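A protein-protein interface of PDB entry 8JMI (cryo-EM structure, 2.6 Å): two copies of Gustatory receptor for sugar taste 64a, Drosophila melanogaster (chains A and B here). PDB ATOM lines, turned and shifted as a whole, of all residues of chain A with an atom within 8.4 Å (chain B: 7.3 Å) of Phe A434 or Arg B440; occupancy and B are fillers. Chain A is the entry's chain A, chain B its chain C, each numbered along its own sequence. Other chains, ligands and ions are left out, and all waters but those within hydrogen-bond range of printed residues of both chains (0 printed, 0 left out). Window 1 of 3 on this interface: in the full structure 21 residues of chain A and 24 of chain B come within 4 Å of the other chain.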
ATOM      1  N   ASP A 333      -7.384  -8.661  24.475  1.00  0.00           N
ATOM      2  CA  ASP A 333      -7.206  -9.027  23.078  1.00  0.00           C
ATOM      3  C   ASP A 333      -5.731  -9.149  22.729  1.00  0.00           C
ATOM      4  O   ASP A 333      -5.326 -10.082  22.032  1.00  0.00           O
ATOM      5  CB  ASP A 333      -7.887  -7.993  22.183  1.00  0.00           C
ATOM      6  CG  ASP A 333      -8.126  -8.503  20.779  1.00  0.00           C
ATOM      7  OD1 ASP A 333      -8.245  -9.733  20.601  1.00  0.00           O
ATOM      8  OD2 ASP A 333      -8.195  -7.671  19.851  1.00  0.00           O
ATOM      9  N   SER A 337      -4.587 -12.790  21.470  1.00  0.00           N
ATOM     10  CA  SER A 337      -4.635 -12.808  20.013  1.00  0.00           C
ATOM     11  C   SER A 337      -4.026 -14.083  19.449  1.00  0.00           C
ATOM     12  O   SER A 337      -4.540 -14.644  18.476  1.00  0.00           O
ATOM     13  CB  SER A 337      -3.921 -11.577  19.459  1.00  0.00           C
ATOM     14  OG  SER A 337      -2.549 -11.585  19.808  1.00  0.00           O
ATOM     15  N   LEU A 341      -6.074 -16.680  17.128  1.00  0.00           N
ATOM     16  CA  LEU A 341      -5.619 -17.038  15.789  1.00  0.00           C
ATOM     17  C   LEU A 341      -5.455 -18.546  15.650  1.00  0.00           C
ATOM     18  O   LEU A 341      -5.900 -19.145  14.661  1.00  0.00           O
ATOM     19  CB  LEU A 341      -4.299 -16.326  15.483  1.00  0.00           C
ATOM     20  CG  LEU A 341      -4.114 -15.649  14.121  1.00  0.00           C
ATOM     21  CD1 LEU A 341      -5.321 -14.817  13.729  1.00  0.00           C
ATOM     22  CD2 LEU A 341      -2.860 -14.792  14.135  1.00  0.00           C
ATOM     23  N   THR A 426     -14.573  -0.333  17.025  1.00  0.00           N
ATOM     24  CA  THR A 426     -14.904  -1.751  16.918  1.00  0.00           C
ATOM     25  C   THR A 426     -14.537  -2.411  18.241  1.00  0.00           C
ATOM     26  O   THR A 426     -13.366  -2.690  18.507  1.00  0.00           O
ATOM     27  CB  THR A 426     -14.170  -2.395  15.748  1.00  0.00           C
ATOM     28  OG1 THR A 426     -14.538  -1.738  14.529  1.00  0.00           O
ATOM     29  CG2 THR A 426     -14.515  -3.876  15.643  1.00  0.00           C
ATOM     30  N   LEU A 429     -13.089  -8.772  20.247  1.00  0.00           N
ATOM     31  CA  LEU A 429     -11.856  -9.542  20.212  1.00  0.00           C
ATOM     32  C   LEU A 429     -11.407  -9.726  18.768  1.00  0.00           C
ATOM     33  O   LEU A 429     -12.222  -9.766  17.843  1.00  0.00           O
ATOM     34  CB  LEU A 429     -12.056 -10.903  20.883  1.00  0.00           C
ATOM     35  CG  LEU A 429     -12.272 -10.906  22.399  1.00  0.00           C
ATOM     36  CD1 LEU A 429     -12.586 -12.310  22.886  1.00  0.00           C
ATOM     37  CD2 LEU A 429     -11.059 -10.351  23.129  1.00  0.00           C
ATOM     38  N   SER A 430     -10.095  -9.830  18.575  1.00  0.00           N
ATOM     39  CA  SER A 430      -9.524  -9.888  17.238  1.00  0.00           C
ATOM     40  C   SER A 430      -8.422 -10.933  17.190  1.00  0.00           C
ATOM     41  O   SER A 430      -7.786 -11.239  18.201  1.00  0.00           O
ATOM     42  CB  SER A 430      -8.961  -8.527  16.808  1.00  0.00           C
ATOM     43  OG  SER A 430      -7.718  -8.270  17.434  1.00  0.00           O
ATOM     44  N   GLY A 431      -8.211 -11.480  15.996  1.00  0.00           N
ATOM     45  CA  GLY A 431      -7.100 -12.374  15.745  1.00  0.00           C
ATOM     46  C   GLY A 431      -5.859 -11.621  15.310  1.00  0.00           C
ATOM     47  O   GLY A 431      -5.506 -11.635  14.127  1.00  0.00           O
ATOM     48  N   LYS A 432      -5.196 -10.952  16.252  1.00  0.00           N
ATOM     49  CA  LYS A 432      -4.028 -10.119  15.960  1.00  0.00           C
ATOM     50  C   LYS A 432      -4.386  -8.972  15.021  1.00  0.00           C
ATOM     51  O   LYS A 432      -3.561  -8.528  14.218  1.00  0.00           O
ATOM     52  CB  LYS A 432      -2.880 -10.951  15.378  1.00  0.00           C
ATOM     53  CG  LYS A 432      -2.009 -11.629  16.423  1.00  0.00           C
ATOM     54  CD  LYS A 432      -0.546 -11.268  16.255  1.00  0.00           C
ATOM     55  CE  LYS A 432       0.291 -11.775  17.419  1.00  0.00           C
ATOM     56  NZ  LYS A 432      -0.202 -13.072  17.963  1.00  0.00           N
ATOM     57  N   LYS A 433      -5.621  -8.485  15.115  1.00  0.00           N
ATOM     58  CA  LYS A 433      -6.140  -7.384  14.310  1.00  0.00           C
ATOM     59  C   LYS A 433      -6.199  -7.717  12.824  1.00  0.00           C
ATOM     60  O   LYS A 433      -6.444  -6.825  12.004  1.00  0.00           O
ATOM     61  CB  LYS A 433      -5.328  -6.101  14.525  1.00  0.00           C
ATOM     62  CG  LYS A 433      -5.772  -5.287  15.732  1.00  0.00           C
ATOM     63  CD  LYS A 433      -4.751  -5.345  16.855  1.00  0.00           C
ATOM     64  CE  LYS A 433      -5.095  -4.377  17.979  1.00  0.00           C
ATOM     65  NZ  LYS A 433      -6.563  -4.192  18.145  1.00  0.00           N
ATOM     66  N   PHE A 434      -5.981  -8.980  12.452  1.00  0.00           N
ATOM     67  CA  PHE A 434      -6.200  -9.386  11.070  1.00  0.00           C
ATOM     68  C   PHE A 434      -7.686  -9.483  10.764  1.00  0.00           C
ATOM     69  O   PHE A 434      -8.108  -9.239   9.629  1.00  0.00           O
ATOM     70  CB  PHE A 434      -5.518 -10.726  10.805  1.00  0.00           C
ATOM     71  CG  PHE A 434      -4.024 -10.671  10.899  1.00  0.00           C
ATOM     72  CD1 PHE A 434      -3.291  -9.866  10.045  1.00  0.00           C
ATOM     73  CD2 PHE A 434      -3.351 -11.424  11.844  1.00  0.00           C
ATOM     74  CE1 PHE A 434      -1.916  -9.814  10.132  1.00  0.00           C
ATOM     75  CE2 PHE A 434      -1.977 -11.377  11.935  1.00  0.00           C
ATOM     76  CZ  PHE A 434      -1.258 -10.572  11.078  1.00  0.00           C
ATOM     77  N   TYR A 435      -8.483  -9.839  11.766  1.00  0.00           N
ATOM     78  CA  TYR A 435      -9.931  -9.896  11.659  1.00  0.00           C
ATOM     79  C   TYR A 435     -10.494  -9.696  13.056  1.00  0.00           C
ATOM     80  O   TYR A 435      -9.789  -9.863  14.054  1.00  0.00           O
ATOM     81  CB  TYR A 435     -10.402 -11.227  11.064  1.00  0.00           C
ATOM     82  CG  TYR A 435      -9.874 -12.434  11.803  1.00  0.00           C
ATOM     83  CD1 TYR A 435     -10.579 -12.987  12.864  1.00  0.00           C
ATOM     84  CD2 TYR A 435      -8.665 -13.016  11.449  1.00  0.00           C
ATOM     85  CE1 TYR A 435     -10.099 -14.086  13.545  1.00  0.00           C
ATOM     86  CE2 TYR A 435      -8.177 -14.116  12.122  1.00  0.00           C
ATOM     87  CZ  TYR A 435      -8.898 -14.648  13.170  1.00  0.00           C
ATOM     88  OH  TYR A 435      -8.414 -15.743  13.846  1.00  0.00           O
ATOM     89  N   PHE A 436     -11.770  -9.335  13.118  1.00  0.00           N
ATOM     90  CA  PHE A 436     -12.445  -9.073  14.381  1.00  0.00           C
ATOM     91  C   PHE A 436     -13.604 -10.044  14.548  1.00  0.00           C
ATOM     92  O   PHE A 436     -14.376 -10.265  13.610  1.00  0.00           O
ATOM     93  CB  PHE A 436     -12.936  -7.628  14.444  1.00  0.00           C
ATOM     94  CG  PHE A 436     -11.843  -6.641  14.709  1.00  0.00           C
ATOM     95  CD1 PHE A 436     -11.034  -6.194  13.679  1.00  0.00           C
ATOM     96  CD2 PHE A 436     -11.611  -6.171  15.990  1.00  0.00           C
ATOM     97  CE1 PHE A 436     -10.020  -5.291  13.919  1.00  0.00           C
ATOM     98  CE2 PHE A 436     -10.598  -5.266  16.236  1.00  0.00           C
ATOM     99  CZ  PHE A 436      -9.801  -4.826  15.198  1.00  0.00           C
ATOM    100  N   LEU A 437     -13.722 -10.616  15.745  1.00  0.00           N
ATOM    101  CA  LEU A 437     -14.752 -11.608  16.016  1.00  0.00           C
ATOM    102  C   LEU A 437     -16.116 -10.941  16.116  1.00  0.00           C
ATOM    103  O   LEU A 437     -16.503 -10.450  17.180  1.00  0.00           O
ATOM    104  CB  LEU A 437     -14.427 -12.379  17.298  1.00  0.00           C
ATOM    105  CG  LEU A 437     -13.103 -13.150  17.279  1.00  0.00           C
ATOM    106  CD1 LEU A 437     -12.860 -13.852  18.604  1.00  0.00           C
ATOM    107  CD2 LEU A 437     -13.080 -14.154  16.139  1.00  0.00           C
ATOM    108  N   THR A 438     -16.843 -10.915  15.002  1.00  0.00           N
ATOM    109  CA  THR A 438     -18.168 -10.324  14.925  1.00  0.00           C
ATOM    110  C   THR A 438     -19.097 -11.287  14.198  1.00  0.00           C
ATOM    111  O   THR A 438     -18.665 -12.296  13.636  1.00  0.00           O
ATOM    112  CB  THR A 438     -18.136  -8.968  14.205  1.00  0.00           C
ATOM    113  OG1 THR A 438     -17.703  -9.150  12.852  1.00  0.00           O
ATOM    114  CG2 THR A 438     -17.187  -8.007  14.910  1.00  0.00           C
ATOM    115  N   LEU A 441     -18.125 -11.458  10.700  1.00  0.00           N
ATOM    116  CA  LEU A 441     -16.990 -12.349  10.490  1.00  0.00           C
ATOM    117  C   LEU A 441     -17.433 -13.804  10.458  1.00  0.00           C
ATOM    118  O   LEU A 441     -16.902 -14.597   9.677  1.00  0.00           O
ATOM    119  CB  LEU A 441     -15.932 -12.139  11.573  1.00  0.00           C
ATOM    120  CG  LEU A 441     -14.683 -13.012  11.403  1.00  0.00           C
ATOM    121  CD1 LEU A 441     -13.767 -12.421  10.344  1.00  0.00           C
ATOM    122  CD2 LEU A 441     -13.941 -13.185  12.716  1.00  0.00           C
ATOM    123  N   ALA B 383       4.715 -11.024   4.059  1.00  0.00           N
ATOM    124  CA  ALA B 383       4.008 -10.763   5.306  1.00  0.00           C
ATOM    125  C   ALA B 383       4.669  -9.639   6.088  1.00  0.00           C
ATOM    126  O   ALA B 383       3.983  -8.790   6.659  1.00  0.00           O
ATOM    127  CB  ALA B 383       3.947 -12.036   6.149  1.00  0.00           C
ATOM    128  N   LEU B 387       3.065  -6.147   7.045  1.00  0.00           N
ATOM    129  CA  LEU B 387       2.913  -5.836   8.461  1.00  0.00           C
ATOM    130  C   LEU B 387       3.628  -4.542   8.825  1.00  0.00           C
ATOM    131  O   LEU B 387       3.119  -3.753   9.625  1.00  0.00           O
ATOM    132  CB  LEU B 387       3.439  -6.996   9.304  1.00  0.00           C
ATOM    133  CG  LEU B 387       2.589  -8.267   9.279  1.00  0.00           C
ATOM    134  CD1 LEU B 387       3.389  -9.455   9.788  1.00  0.00           C
ATOM    135  CD2 LEU B 387       1.322  -8.082  10.094  1.00  0.00           C
ATOM    136  N   ALA B 390       1.437  -1.828   7.507  1.00  0.00           N
ATOM    137  CA  ALA B 390       0.235  -1.718   8.319  1.00  0.00           C
ATOM    138  C   ALA B 390       0.530  -1.204   9.717  1.00  0.00           C
ATOM    139  O   ALA B 390      -0.391  -0.757  10.407  1.00  0.00           O
ATOM    140  CB  ALA B 390      -0.462  -3.075   8.405  1.00  0.00           C
ATOM    141  N   ASN B 393      -0.708   2.278  10.056  1.00  0.00           N
ATOM    142  CA  ASN B 393      -2.126   2.389  10.382  1.00  0.00           C
ATOM    143  C   ASN B 393      -2.382   2.040  11.842  1.00  0.00           C
ATOM    144  O   ASN B 393      -3.139   2.728  12.540  1.00  0.00           O
ATOM    145  CB  ASN B 393      -2.934   1.477   9.456  1.00  0.00           C
ATOM    146  CG  ASN B 393      -4.428   1.659   9.609  1.00  0.00           C
ATOM    147  OD1 ASN B 393      -5.117   0.791  10.141  1.00  0.00           O
ATOM    148  ND2 ASN B 393      -4.938   2.786   9.131  1.00  0.00           N
ATOM    149  N   GLU B 394      -1.756   0.964  12.322  1.00  0.00           N
ATOM    150  CA  GLU B 394      -1.946   0.557  13.710  1.00  0.00           C
ATOM    151  C   GLU B 394      -1.465   1.639  14.668  1.00  0.00           C
ATOM    152  O   GLU B 394      -2.133   1.939  15.662  1.00  0.00           O
ATOM    153  CB  GLU B 394      -1.218  -0.760  13.981  1.00  0.00           C
ATOM    154  CG  GLU B 394      -1.670  -1.924  13.112  1.00  0.00           C
ATOM    155  CD  GLU B 394      -3.163  -2.172  13.187  1.00  0.00           C
ATOM    156  OE1 GLU B 394      -3.684  -2.346  14.308  1.00  0.00           O
ATOM    157  OE2 GLU B 394      -3.817  -2.195  12.123  1.00  0.00           O
ATOM    158  N   PHE B 436      -5.336  -0.582   0.547  1.00  0.00           N
ATOM    159  CA  PHE B 436      -4.534   0.046   1.586  1.00  0.00           C
ATOM    160  C   PHE B 436      -3.812  -1.024   2.390  1.00  0.00           C
ATOM    161  O   PHE B 436      -4.410  -2.038   2.762  1.00  0.00           O
ATOM    162  CB  PHE B 436      -5.407   0.909   2.497  1.00  0.00           C
ATOM    163  CG  PHE B 436      -5.807   2.211   1.875  1.00  0.00           C
ATOM    164  CD1 PHE B 436      -6.873   2.271   0.994  1.00  0.00           C
ATOM    165  CD2 PHE B 436      -5.108   3.372   2.155  1.00  0.00           C
ATOM    166  CE1 PHE B 436      -7.240   3.465   0.411  1.00  0.00           C
ATOM    167  CE2 PHE B 436      -5.473   4.571   1.576  1.00  0.00           C
ATOM    168  CZ  PHE B 436      -6.540   4.617   0.702  1.00  0.00           C
ATOM    169  N   LEU B 437      -2.529  -0.791   2.657  1.00  0.00           N
ATOM    170  CA  LEU B 437      -1.707  -1.766   3.360  1.00  0.00           C
ATOM    171  C   LEU B 437      -2.070  -1.797   4.837  1.00  0.00           C
ATOM    172  O   LEU B 437      -1.545  -1.012   5.634  1.00  0.00           O
ATOM    173  CB  LEU B 437      -0.221  -1.450   3.169  1.00  0.00           C
ATOM    174  CG  LEU B 437       0.271  -1.461   1.719  1.00  0.00           C
ATOM    175  CD1 LEU B 437       1.745  -1.105   1.639  1.00  0.00           C
ATOM    176  CD2 LEU B 437       0.021  -2.815   1.076  1.00  0.00           C
ATOM    177  N   THR B 438      -2.974  -2.700   5.204  1.00  0.00           N
ATOM    178  CA  THR B 438      -3.430  -2.865   6.575  1.00  0.00           C
ATOM    179  C   THR B 438      -3.403  -4.346   6.927  1.00  0.00           C
ATOM    180  O   THR B 438      -3.198  -5.209   6.070  1.00  0.00           O
ATOM    181  CB  THR B 438      -4.843  -2.296   6.768  1.00  0.00           C
ATOM    182  OG1 THR B 438      -5.770  -3.020   5.951  1.00  0.00           O
ATOM    183  CG2 THR B 438      -4.886  -0.822   6.389  1.00  0.00           C
ATOM    184  N   ARG B 439      -3.608  -4.639   8.213  1.00  0.00           N
ATOM    185  CA  ARG B 439      -3.686  -6.031   8.641  1.00  0.00           C
ATOM    186  C   ARG B 439      -4.868  -6.734   7.988  1.00  0.00           C
ATOM    187  O   ARG B 439      -4.775  -7.913   7.621  1.00  0.00           O
ATOM    188  CB  ARG B 439      -3.790  -6.106  10.163  1.00  0.00           C
ATOM    189  CG  ARG B 439      -2.557  -5.600  10.889  1.00  0.00           C
ATOM    190  CD  ARG B 439      -2.336  -6.319  12.207  1.00  0.00           C
ATOM    191  NE  ARG B 439      -0.972  -6.141  12.690  1.00  0.00           N
ATOM    192  CZ  ARG B 439      -0.251  -7.075  13.296  1.00  0.00           C
ATOM    193  NH1 ARG B 439      -0.735  -8.284  13.530  1.00  0.00           N
ATOM    194  NH2 ARG B 439       0.990  -6.787  13.680  1.00  0.00           N
ATOM    195  N   ARG B 440      -5.987  -6.025   7.835  1.00  0.00           N
ATOM    196  CA  ARG B 440      -7.130  -6.594   7.133  1.00  0.00           C
ATOM    197  C   ARG B 440      -6.769  -6.931   5.693  1.00  0.00           C
ATOM    198  O   ARG B 440      -7.199  -7.960   5.162  1.00  0.00           O
ATOM    199  CB  ARG B 440      -8.309  -5.621   7.173  1.00  0.00           C
ATOM    200  CG  ARG B 440      -8.759  -5.245   8.575  1.00  0.00           C
ATOM    201  CD  ARG B 440     -10.079  -5.903   8.937  1.00  0.00           C
ATOM    202  NE  ARG B 440     -10.014  -7.357   8.819  1.00  0.00           N
ATOM    203  CZ  ARG B 440     -10.852  -8.108   8.113  1.00  0.00           C
ATOM    204  NH1 ARG B 440     -11.855  -7.580   7.430  1.00  0.00           N
ATOM    205  NH2 ARG B 440     -10.677  -9.426   8.092  1.00  0.00           N
ATOM    206  N   LEU B 441      -5.982  -6.071   5.042  1.00  0.00           N
ATOM    207  CA  LEU B 441      -5.562  -6.361   3.676  1.00  0.00           C
ATOM    208  C   LEU B 441      -4.674  -7.596   3.624  1.00  0.00           C
ATOM    209  O   LEU B 441      -4.770  -8.389   2.685  1.00  0.00           O
ATOM    210  CB  LEU B 441      -4.836  -5.161   3.067  1.00  0.00           C
ATOM    211  CG  LEU B 441      -4.396  -5.369   1.613  1.00  0.00           C
ATOM    212  CD1 LEU B 441      -5.574  -5.177   0.673  1.00  0.00           C
ATOM    213  CD2 LEU B 441      -3.253  -4.442   1.237  1.00  0.00           C
ATOM    214  N   LEU B 442      -3.788  -7.769   4.606  1.00  0.00           N
ATOM    215  CA  LEU B 442      -2.946  -8.961   4.621  1.00  0.00           C
ATOM    216  C   LEU B 442      -3.783 -10.216   4.834  1.00  0.00           C
ATOM    217  O   LEU B 442      -3.535 -11.254   4.206  1.00  0.00           O
ATOM    218  CB  LEU B 442      -1.873  -8.833   5.702  1.00  0.00           C
ATOM    219  CG  LEU B 442      -0.816  -9.943   5.763  1.00  0.00           C
ATOM    220  CD1 LEU B 442      -0.203 -10.210   4.393  1.00  0.00           C
ATOM    221  CD2 LEU B 442       0.265  -9.586   6.769  1.00  0.00           C
ATOM    222  N   PHE B 443      -4.785 -10.140   5.712  1.00  0.00           N
ATOM    223  CA  PHE B 443      -5.692 -11.269   5.895  1.00  0.00           C
ATOM    224  C   PHE B 443      -6.438 -11.590   4.605  1.00  0.00           C
ATOM    225  O   PHE B 443      -6.566 -12.761   4.220  1.00  0.00           O
ATOM    226  CB  PHE B 443      -6.678 -10.956   7.020  1.00  0.00           C
ATOM    227  CG  PHE B 443      -7.566 -12.109   7.392  1.00  0.00           C
ATOM    228  CD1 PHE B 443      -7.026 -13.308   7.821  1.00  0.00           C
ATOM    229  CD2 PHE B 443      -8.941 -11.987   7.321  1.00  0.00           C
ATOM    230  CE1 PHE B 443      -7.842 -14.366   8.165  1.00  0.00           C
ATOM    231  CE2 PHE B 443      -9.763 -13.041   7.665  1.00  0.00           C
ATOM    232  CZ  PHE B 443      -9.213 -14.232   8.088  1.00  0.00           C
ATOM    233  N   GLY B 444      -6.936 -10.559   3.921  1.00  0.00           N
ATOM    234  CA  GLY B 444      -7.628 -10.783   2.663  1.00  0.00           C
ATOM    235  C   GLY B 444      -6.715 -11.343   1.592  1.00  0.00           C
ATOM    236  O   GLY B 444      -7.131 -12.168   0.779  1.00  0.00           O
ATOM    237  N   MET B 445      -5.456 -10.903   1.578  1.00  0.00           N
ATOM    238  CA  MET B 445      -4.487 -11.450   0.636  1.00  0.00           C
ATOM    239  C   MET B 445      -4.223 -12.920   0.921  1.00  0.00           C
ATOM    240  O   MET B 445      -4.115 -13.728  -0.006  1.00  0.00           O
ATOM    241  CB  MET B 445      -3.185 -10.652   0.702  1.00  0.00           C
ATOM    242  CG  MET B 445      -2.303 -10.801  -0.528  1.00  0.00           C
ATOM    243  SD  MET B 445      -0.546 -10.707  -0.141  1.00  0.00           S
ATOM    244  CE  MET B 445       0.163 -10.623  -1.784  1.00  0.00           C
ATOM    245  N   ALA B 446      -4.109 -13.287   2.198  1.00  0.00           N
ATOM    246  CA  ALA B 446      -3.940 -14.695   2.539  1.00  0.00           C
ATOM    247  C   ALA B 446      -5.142 -15.514   2.085  1.00  0.00           C
ATOM    248  O   ALA B 446      -4.985 -16.604   1.522  1.00  0.00           O
ATOM    249  CB  ALA B 446      -3.724 -14.848   4.044  1.00  0.00           C
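Of the printed residues of chain B, Phe A434 touches Leu B387 (3.7 Å), Arg B439 (3.4 Å), Arg B440 (2.8 Å) and Phe B443 (3.4 Å). Printed residues of chain A within 4 Å of Arg B439: Lys A432, Lys A433 and Phe A434. Arg B440 touches two residues of chain A. Of the printed residues of chain A, Phe B443 touches Phe A434 (3.4 Å) and Tyr A435 (3.6 Å). The nearest printed residue of chain B that does not touch Phe A434 is Leu B442 (4.01 Å). The nearest printed residue of chain A that does not touch Glu B394 is Lys A432 (6.2 Å).
The side-chain hydroxyl (OG) of Ser A337 sits at hydrogen-bond distance from the side-chain amino group (NZ) of Lys A432 (3.3 Å). The side-chain hydroxyl of Ser A430 sits at hydrogen-bond distance from the backbone NH of Lys A433 (3.1 Å).
Among the printed residues, merely in contact across the chains: Lys A433 with Glu B394, Lys A433 with Arg B439, Phe A434 with Leu B387, Phe A434 with Arg B439, Phe A434 with Phe B443, Tyr A435 with Arg B440 and Tyr A435 with Phe B443.
The guanidinium group of Arg B439 lies within hydrogen-bond range of the backbone carbonyl oxygen of Lys A432 (2.9 Å). O of Phe A434 sits at hydrogen-bond distance from NE of Arg B440 (2.8 Å).
Of the 16 printed residues of chain B, 5 touch a printed residue of chain A. Hydrophobic or aromatic side chains of chain B within 4 Å of the printed part of chain A: Leu B387 and Phe B443. Of the 15 printed residues of chain A, 4 touch a printed residue of chain B. Hydrophobic or aromatic side chains of chain A that line the printed part of chain B: Phe A434 and Tyr A435. Along chain A the printed residues that touch a printed residue of chain B span positions 432 to 435. Among the printed residues, no Asp or Glu carboxylate lies within 4 Å of a Lys or Arg side-chain nitrogen of the other chain.
4 positions are printed for both chains.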
